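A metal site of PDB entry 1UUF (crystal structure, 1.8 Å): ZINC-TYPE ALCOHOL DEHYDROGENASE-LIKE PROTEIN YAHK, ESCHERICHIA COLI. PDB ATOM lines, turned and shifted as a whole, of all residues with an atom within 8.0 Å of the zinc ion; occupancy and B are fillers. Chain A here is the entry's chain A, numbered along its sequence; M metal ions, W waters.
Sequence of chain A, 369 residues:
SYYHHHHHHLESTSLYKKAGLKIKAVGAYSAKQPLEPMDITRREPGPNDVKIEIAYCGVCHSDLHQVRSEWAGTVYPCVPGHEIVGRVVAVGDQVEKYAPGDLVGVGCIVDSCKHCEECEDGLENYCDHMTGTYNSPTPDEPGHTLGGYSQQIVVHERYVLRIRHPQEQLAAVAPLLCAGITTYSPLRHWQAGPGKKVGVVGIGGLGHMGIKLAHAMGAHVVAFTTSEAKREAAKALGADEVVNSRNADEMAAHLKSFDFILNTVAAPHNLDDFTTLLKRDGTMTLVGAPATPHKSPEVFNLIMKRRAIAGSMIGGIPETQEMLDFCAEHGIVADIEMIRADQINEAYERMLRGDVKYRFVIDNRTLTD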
ATOM      1  N   GLY A  58      -3.976  22.397  -5.122  1.00  0.00           N
ATOM      2  CA  GLY A  58      -3.128  23.313  -4.389  1.00  0.00           C
ATOM      3  C   GLY A  58      -3.330  24.739  -4.890  1.00  0.00           C
ATOM      4  O   GLY A  58      -3.703  24.956  -6.037  1.00  0.00           O
ATOM      5  N   VAL A  59      -3.090  25.710  -4.017  1.00  0.00           N
ATOM      6  CA  VAL A  59      -3.240  27.110  -4.389  1.00  0.00           C
ATOM      7  C   VAL A  59      -1.855  27.692  -4.637  1.00  0.00           C
ATOM      8  O   VAL A  59      -1.005  27.730  -3.743  1.00  0.00           O
ATOM      9  CB  VAL A  59      -3.961  27.890  -3.268  1.00  0.00           C
ATOM     10  CG1 VAL A  59      -4.138  29.346  -3.685  1.00  0.00           C
ATOM     11  CG2 VAL A  59      -5.319  27.251  -2.975  1.00  0.00           C
ATOM     12  N   CYS A  60      -1.633  28.129  -5.876  1.00  0.00           N
ATOM     13  CA  CYS A  60      -0.344  28.671  -6.303  1.00  0.00           C
ATOM     14  C   CYS A  60      -0.407  30.181  -6.486  1.00  0.00           C
ATOM     15  O   CYS A  60      -1.466  30.738  -6.775  1.00  0.00           O
ATOM     16  CB  CYS A  60       0.070  28.016  -7.626  1.00  0.00           C
ATOM     17  SG  CYS A  60       1.639  28.612  -8.308  1.00  0.00           S
ATOM     18  N   HIS A  61       0.730  30.851  -6.308  1.00  0.00           N
ATOM     19  CA  HIS A  61       0.754  32.300  -6.483  1.00  0.00           C
ATOM     20  C   HIS A  61       0.365  32.668  -7.915  1.00  0.00           C
ATOM     21  O   HIS A  61      -0.116  33.783  -8.162  1.00  0.00           O
ATOM     22  CB  HIS A  61       2.133  32.865  -6.140  1.00  0.00           C
ATOM     23  CG  HIS A  61       2.323  33.171  -4.683  1.00  0.00           C
ATOM     24  ND1 HIS A  61       2.562  32.188  -3.748  1.00  0.00           N
ATOM     25  CD2 HIS A  61       2.259  34.342  -4.008  1.00  0.00           C
ATOM     26  CE1 HIS A  61       2.647  32.750  -2.548  1.00  0.00           C
ATOM     27  NE2 HIS A  61       2.467  34.052  -2.686  1.00  0.00           N
ATOM     28  N   SER A  62       0.568  31.756  -8.854  1.00  0.00           N
ATOM     29  CA  SER A  62       0.194  32.050 -10.229  1.00  0.00           C
ATOM     30  C   SER A  62      -1.317  32.169 -10.366  1.00  0.00           C
ATOM     31  O   SER A  62      -1.814  32.875 -11.249  1.00  0.00           O
ATOM     32  CB  SER A  62       0.715  30.961 -11.179  1.00  0.00           C
ATOM     33  OG  SER A  62       2.123  31.059 -11.311  1.00  0.00           O
ATOM     34  N   ASP A  63      -2.059  31.493  -9.482  1.00  0.00           N
ATOM     35  CA  ASP A  63      -3.521  31.560  -9.521  1.00  0.00           C
ATOM     36  C   ASP A  63      -3.931  32.969  -9.121  1.00  0.00           C
ATOM     37  O   ASP A  63      -4.750  33.615  -9.777  1.00  0.00           O
ATOM     38  CB  ASP A  63      -4.159  30.587  -8.518  1.00  0.00           C
ATOM     39  CG  ASP A  63      -3.793  29.143  -8.790  1.00  0.00           C
ATOM     40  OD1 ASP A  63      -3.421  28.796  -9.930  1.00  0.00           O
ATOM     41  OD2 ASP A  63      -3.906  28.325  -7.836  1.00  0.00           O
ATOM     42  N   GLY A  81      -6.032  27.279 -10.691  1.00  0.00           N
ATOM     43  CA  GLY A  81      -5.763  25.976 -10.124  1.00  0.00           C
ATOM     44  C   GLY A  81      -5.017  25.040 -11.058  1.00  0.00           C
ATOM     45  O   GLY A  81      -5.537  24.657 -12.096  1.00  0.00           O
ATOM     46  N   HIS A  82      -3.787  24.682 -10.699  1.00  0.00           N
ATOM     47  CA  HIS A  82      -3.032  23.755 -11.526  1.00  0.00           C
ATOM     48  C   HIS A  82      -2.070  22.864 -10.742  1.00  0.00           C
ATOM     49  O   HIS A  82      -0.984  22.533 -11.208  1.00  0.00           O
ATOM     50  CB  HIS A  82      -2.328  24.465 -12.688  1.00  0.00           C
ATOM     51  CG  HIS A  82      -1.387  25.565 -12.281  1.00  0.00           C
ATOM     52  ND1 HIS A  82      -1.031  26.579 -13.152  1.00  0.00           N
ATOM     53  CD2 HIS A  82      -0.702  25.790 -11.133  1.00  0.00           C
ATOM     54  CE1 HIS A  82      -0.161  27.383 -12.550  1.00  0.00           C
ATOM     55  NE2 HIS A  82       0.048  26.925 -11.332  1.00  0.00           N
ATOM     56  N   GLU A  83      -2.496  22.479  -9.541  1.00  0.00           N
ATOM     57  CA  GLU A  83      -1.775  21.566  -8.666  1.00  0.00           C
ATOM     58  C   GLU A  83      -2.906  20.617  -8.307  1.00  0.00           C
ATOM     59  O   GLU A  83      -3.375  20.558  -7.173  1.00  0.00           O
ATOM     60  CB  GLU A  83      -1.239  22.302  -7.422  1.00  0.00           C
ATOM     61  CG  GLU A  83      -0.197  23.369  -7.760  1.00  0.00           C
ATOM     62  CD  GLU A  83       0.566  23.871  -6.544  1.00  0.00           C
ATOM     63  OE1 GLU A  83      -0.036  23.942  -5.453  1.00  0.00           O
ATOM     64  OE2 GLU A  83       1.762  24.206  -6.686  1.00  0.00           O
ATOM     65  N   GLY A 107      -0.636  19.001 -13.745  1.00  0.00           N
ATOM     66  CA  GLY A 107       0.097  20.193 -13.363  1.00  0.00           C
ATOM     67  C   GLY A 107      -0.317  21.420 -14.160  1.00  0.00           C
ATOM     68  O   GLY A 107      -1.513  21.652 -14.398  1.00  0.00           O
ATOM     69  N   CYS A 108       0.670  22.202 -14.592  1.00  0.00           N
ATOM     70  CA  CYS A 108       0.414  23.436 -15.345  1.00  0.00           C
ATOM     71  C   CYS A 108       0.167  23.250 -16.835  1.00  0.00           C
ATOM     72  O   CYS A 108      -0.266  24.182 -17.508  1.00  0.00           O
ATOM     73  CB  CYS A 108       1.596  24.393 -15.186  1.00  0.00           C
ATOM     74  SG  CYS A 108       1.937  24.883 -13.493  1.00  0.00           S
ATOM     75  N   TYR A 134      -4.897  26.577 -17.318  1.00  0.00           N
ATOM     76  CA  TYR A 134      -5.895  27.642 -17.321  1.00  0.00           C
ATOM     77  C   TYR A 134      -5.382  28.863 -18.090  1.00  0.00           C
ATOM     78  O   TYR A 134      -4.180  29.132 -18.131  1.00  0.00           O
ATOM     79  CB  TYR A 134      -6.337  28.037 -15.898  1.00  0.00           C
ATOM     80  CG  TYR A 134      -5.263  28.496 -14.939  1.00  0.00           C
ATOM     81  CD1 TYR A 134      -4.700  29.776 -15.050  1.00  0.00           C
ATOM     82  CD2 TYR A 134      -4.841  27.684 -13.895  1.00  0.00           C
ATOM     83  CE1 TYR A 134      -3.750  30.215 -14.127  1.00  0.00           C
ATOM     84  CE2 TYR A 134      -3.896  28.112 -12.978  1.00  0.00           C
ATOM     85  CZ  TYR A 134      -3.364  29.383 -13.091  1.00  0.00           C
ATOM     86  OH  TYR A 134      -2.432  29.805 -12.169  1.00  0.00           O
ATOM     87  N   PRO A 175       0.424  19.945  -4.143  1.00  0.00           N
ATOM     88  CA  PRO A 175       1.414  20.988  -4.450  1.00  0.00           C
ATOM     89  C   PRO A 175       2.632  20.523  -5.252  1.00  0.00           C
ATOM     90  O   PRO A 175       3.346  21.333  -5.843  1.00  0.00           O
ATOM     91  CB  PRO A 175       1.786  21.522  -3.076  1.00  0.00           C
ATOM     92  CG  PRO A 175       0.550  21.266  -2.254  1.00  0.00           C
ATOM     93  CD  PRO A 175       0.194  19.863  -2.694  1.00  0.00           C
ATOM     94  N   LEU A 177       2.622  19.017  -7.955  1.00  0.00           N
ATOM     95  CA  LEU A 177       2.337  19.232  -9.373  1.00  0.00           C
ATOM     96  C   LEU A 177       2.815  20.552  -9.975  1.00  0.00           C
ATOM     97  O   LEU A 177       2.857  20.712 -11.193  1.00  0.00           O
ATOM     98  CB  LEU A 177       0.838  19.018  -9.633  1.00  0.00           C
ATOM     99  CG  LEU A 177       0.405  17.540  -9.737  1.00  0.00           C
ATOM    100  CD1 LEU A 177       1.113  16.877 -10.910  1.00  0.00           C
ATOM    101  CD2 LEU A 177       0.730  16.809  -8.442  1.00  0.00           C
ATOM    102  N   CYS A 178       3.140  21.521  -9.119  1.00  0.00           N
ATOM    103  CA  CYS A 178       3.696  22.786  -9.614  1.00  0.00           C
ATOM    104  C   CYS A 178       4.846  23.218  -8.717  1.00  0.00           C
ATOM    105  O   CYS A 178       5.989  23.245  -9.161  1.00  0.00           O
ATOM    106  CB  CYS A 178       2.656  23.906  -9.679  1.00  0.00           C
ATOM    107  SG  CYS A 178       3.449  25.428 -10.350  1.00  0.00           S
ATOM    108  N   ALA A 179       4.543  23.550  -7.470  1.00  0.00           N
ATOM    109  CA  ALA A 179       5.584  23.973  -6.545  1.00  0.00           C
ATOM    110  C   ALA A 179       6.697  22.926  -6.508  1.00  0.00           C
ATOM    111  O   ALA A 179       7.882  23.256  -6.511  1.00  0.00           O
ATOM    112  CB  ALA A 179       5.007  24.184  -5.153  1.00  0.00           C
ATOM    113  N   ILE A 181       7.567  20.332  -8.823  1.00  0.00           N
ATOM    114  CA  ILE A 181       8.360  20.222 -10.041  1.00  0.00           C
ATOM    115  C   ILE A 181       9.150  21.495 -10.356  1.00  0.00           C
ATOM    116  O   ILE A 181      10.252  21.424 -10.893  1.00  0.00           O
ATOM    117  CB  ILE A 181       7.477  19.811 -11.253  1.00  0.00           C
ATOM    118  CG1 ILE A 181       8.342  19.610 -12.490  1.00  0.00           C
ATOM    119  CG2 ILE A 181       6.414  20.860 -11.495  1.00  0.00           C
ATOM    120  CD1 ILE A 181       9.400  18.521 -12.353  1.00  0.00           C
ATOM    121  N   THR A 182       8.595  22.645 -10.006  1.00  0.00           N
ATOM    122  CA  THR A 182       9.286  23.916 -10.266  1.00  0.00           C
ATOM    123  C   THR A 182      10.651  23.951  -9.580  1.00  0.00           C
ATOM    124  O   THR A 182      11.597  24.568 -10.095  1.00  0.00           O
ATOM    125  CB  THR A 182       8.437  25.109  -9.809  1.00  0.00           C
ATOM    126  OG1 THR A 182       7.277  25.188 -10.654  1.00  0.00           O
ATOM    127  CG2 THR A 182       9.214  26.418  -9.894  1.00  0.00           C
ATOM    128  N   LEU A 206       7.284  27.550  -2.571  1.00  0.00           N
ATOM    129  CA  LEU A 206       8.348  27.015  -3.415  1.00  0.00           C
ATOM    130  C   LEU A 206       9.565  26.675  -2.576  1.00  0.00           C
ATOM    131  O   LEU A 206      10.155  25.607  -2.731  1.00  0.00           O
ATOM    132  CB  LEU A 206       8.751  28.027  -4.482  1.00  0.00           C
ATOM    133  CG  LEU A 206       7.774  28.292  -5.634  1.00  0.00           C
ATOM    134  CD1 LEU A 206       8.324  29.403  -6.518  1.00  0.00           C
ATOM    135  CD2 LEU A 206       7.583  27.020  -6.441  1.00  0.00           C
ATOM    136  N   ILE A 314       8.559  25.302 -14.006  1.00  0.00           N
ATOM    137  CA  ILE A 314       7.987  23.971 -13.872  1.00  0.00           C
ATOM    138  C   ILE A 314       8.906  22.875 -14.416  1.00  0.00           C
ATOM    139  O   ILE A 314      10.102  22.881 -14.140  1.00  0.00           O
ATOM    140  CB  ILE A 314       6.583  23.880 -14.513  1.00  0.00           C
ATOM    141  CG1 ILE A 314       6.623  24.286 -15.990  1.00  0.00           C
ATOM    142  CG2 ILE A 314       5.637  24.771 -13.739  1.00  0.00           C
ATOM    143  CD1 ILE A 314       5.275  24.140 -16.686  1.00  0.00           C
ATOM    144  N   ARG A 359       1.578  25.571   2.151  1.00  0.00           N
ATOM    145  CA  ARG A 359       0.774  25.561   0.938  1.00  0.00           C
ATOM    146  C   ARG A 359      -0.688  25.314   1.256  1.00  0.00           C
ATOM    147  O   ARG A 359      -1.026  24.419   2.019  1.00  0.00           O
ATOM    148  CB  ARG A 359       1.268  24.446   0.014  1.00  0.00           C
ATOM    149  CG  ARG A 359       1.872  24.906  -1.312  1.00  0.00           C
ATOM    150  CD  ARG A 359       0.797  25.403  -2.260  1.00  0.00           C
ATOM    151  NE  ARG A 359       1.305  25.605  -3.620  1.00  0.00           N
ATOM    152  CZ  ARG A 359       2.126  26.594  -3.968  1.00  0.00           C
ATOM    153  NH1 ARG A 359       2.540  27.473  -3.070  1.00  0.00           N
ATOM    154  NH2 ARG A 359       2.529  26.696  -5.231  1.00  0.00           N
HETATM  155 ZN    ZN M   1       1.895  27.256 -10.228  1.00  0.00          ZN
HETATM  156  O   HOH W   1       3.097  28.613 -11.631  1.00  0.00           O
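A ring nitrogen (ND1) of His 82 sits close to the side-chain sulfur of Cys 108 (3.4 Å). The side-chain sulfur of Cys 60 sits close to the backbone NH of Ser 62 (3.4 Å). The side-chain sulfur (SG) of Cys 60 lies close to the guanidinium group (NH2) of Arg 359. OD2 of Asp 63 lies within hydrogen-bond range of N of Cys 60, 3.0 Å away. The side-chain sulfur of Cys 108 sits close to the side-chain sulfur of Cys 178 (3.5 Å). O of Cys 178 is in hydrogen-bond range of OG1 of Thr 182 (2.8 Å). The backbone carbonyl oxygen (O) of Ser 62 sits close to the side-chain hydroxyl (OH) of Tyr 134, 3.3 Å away.
Residues that only touch the zinc ion: Ser 62 (3.96 Å). Of the 21 residues printed, 4 come within 4 Å of the zinc ion.
NE2 of His 82 binds the zinc ion, at 2.2 Å. The zinc ion is bound by water W1 (2.3 Å). The zinc ion is bound by the side-chain sulfur (SG) of Cys 60 (2.4 Å). The zinc ion is bound by SG of Cys 178 (2.4 Å).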
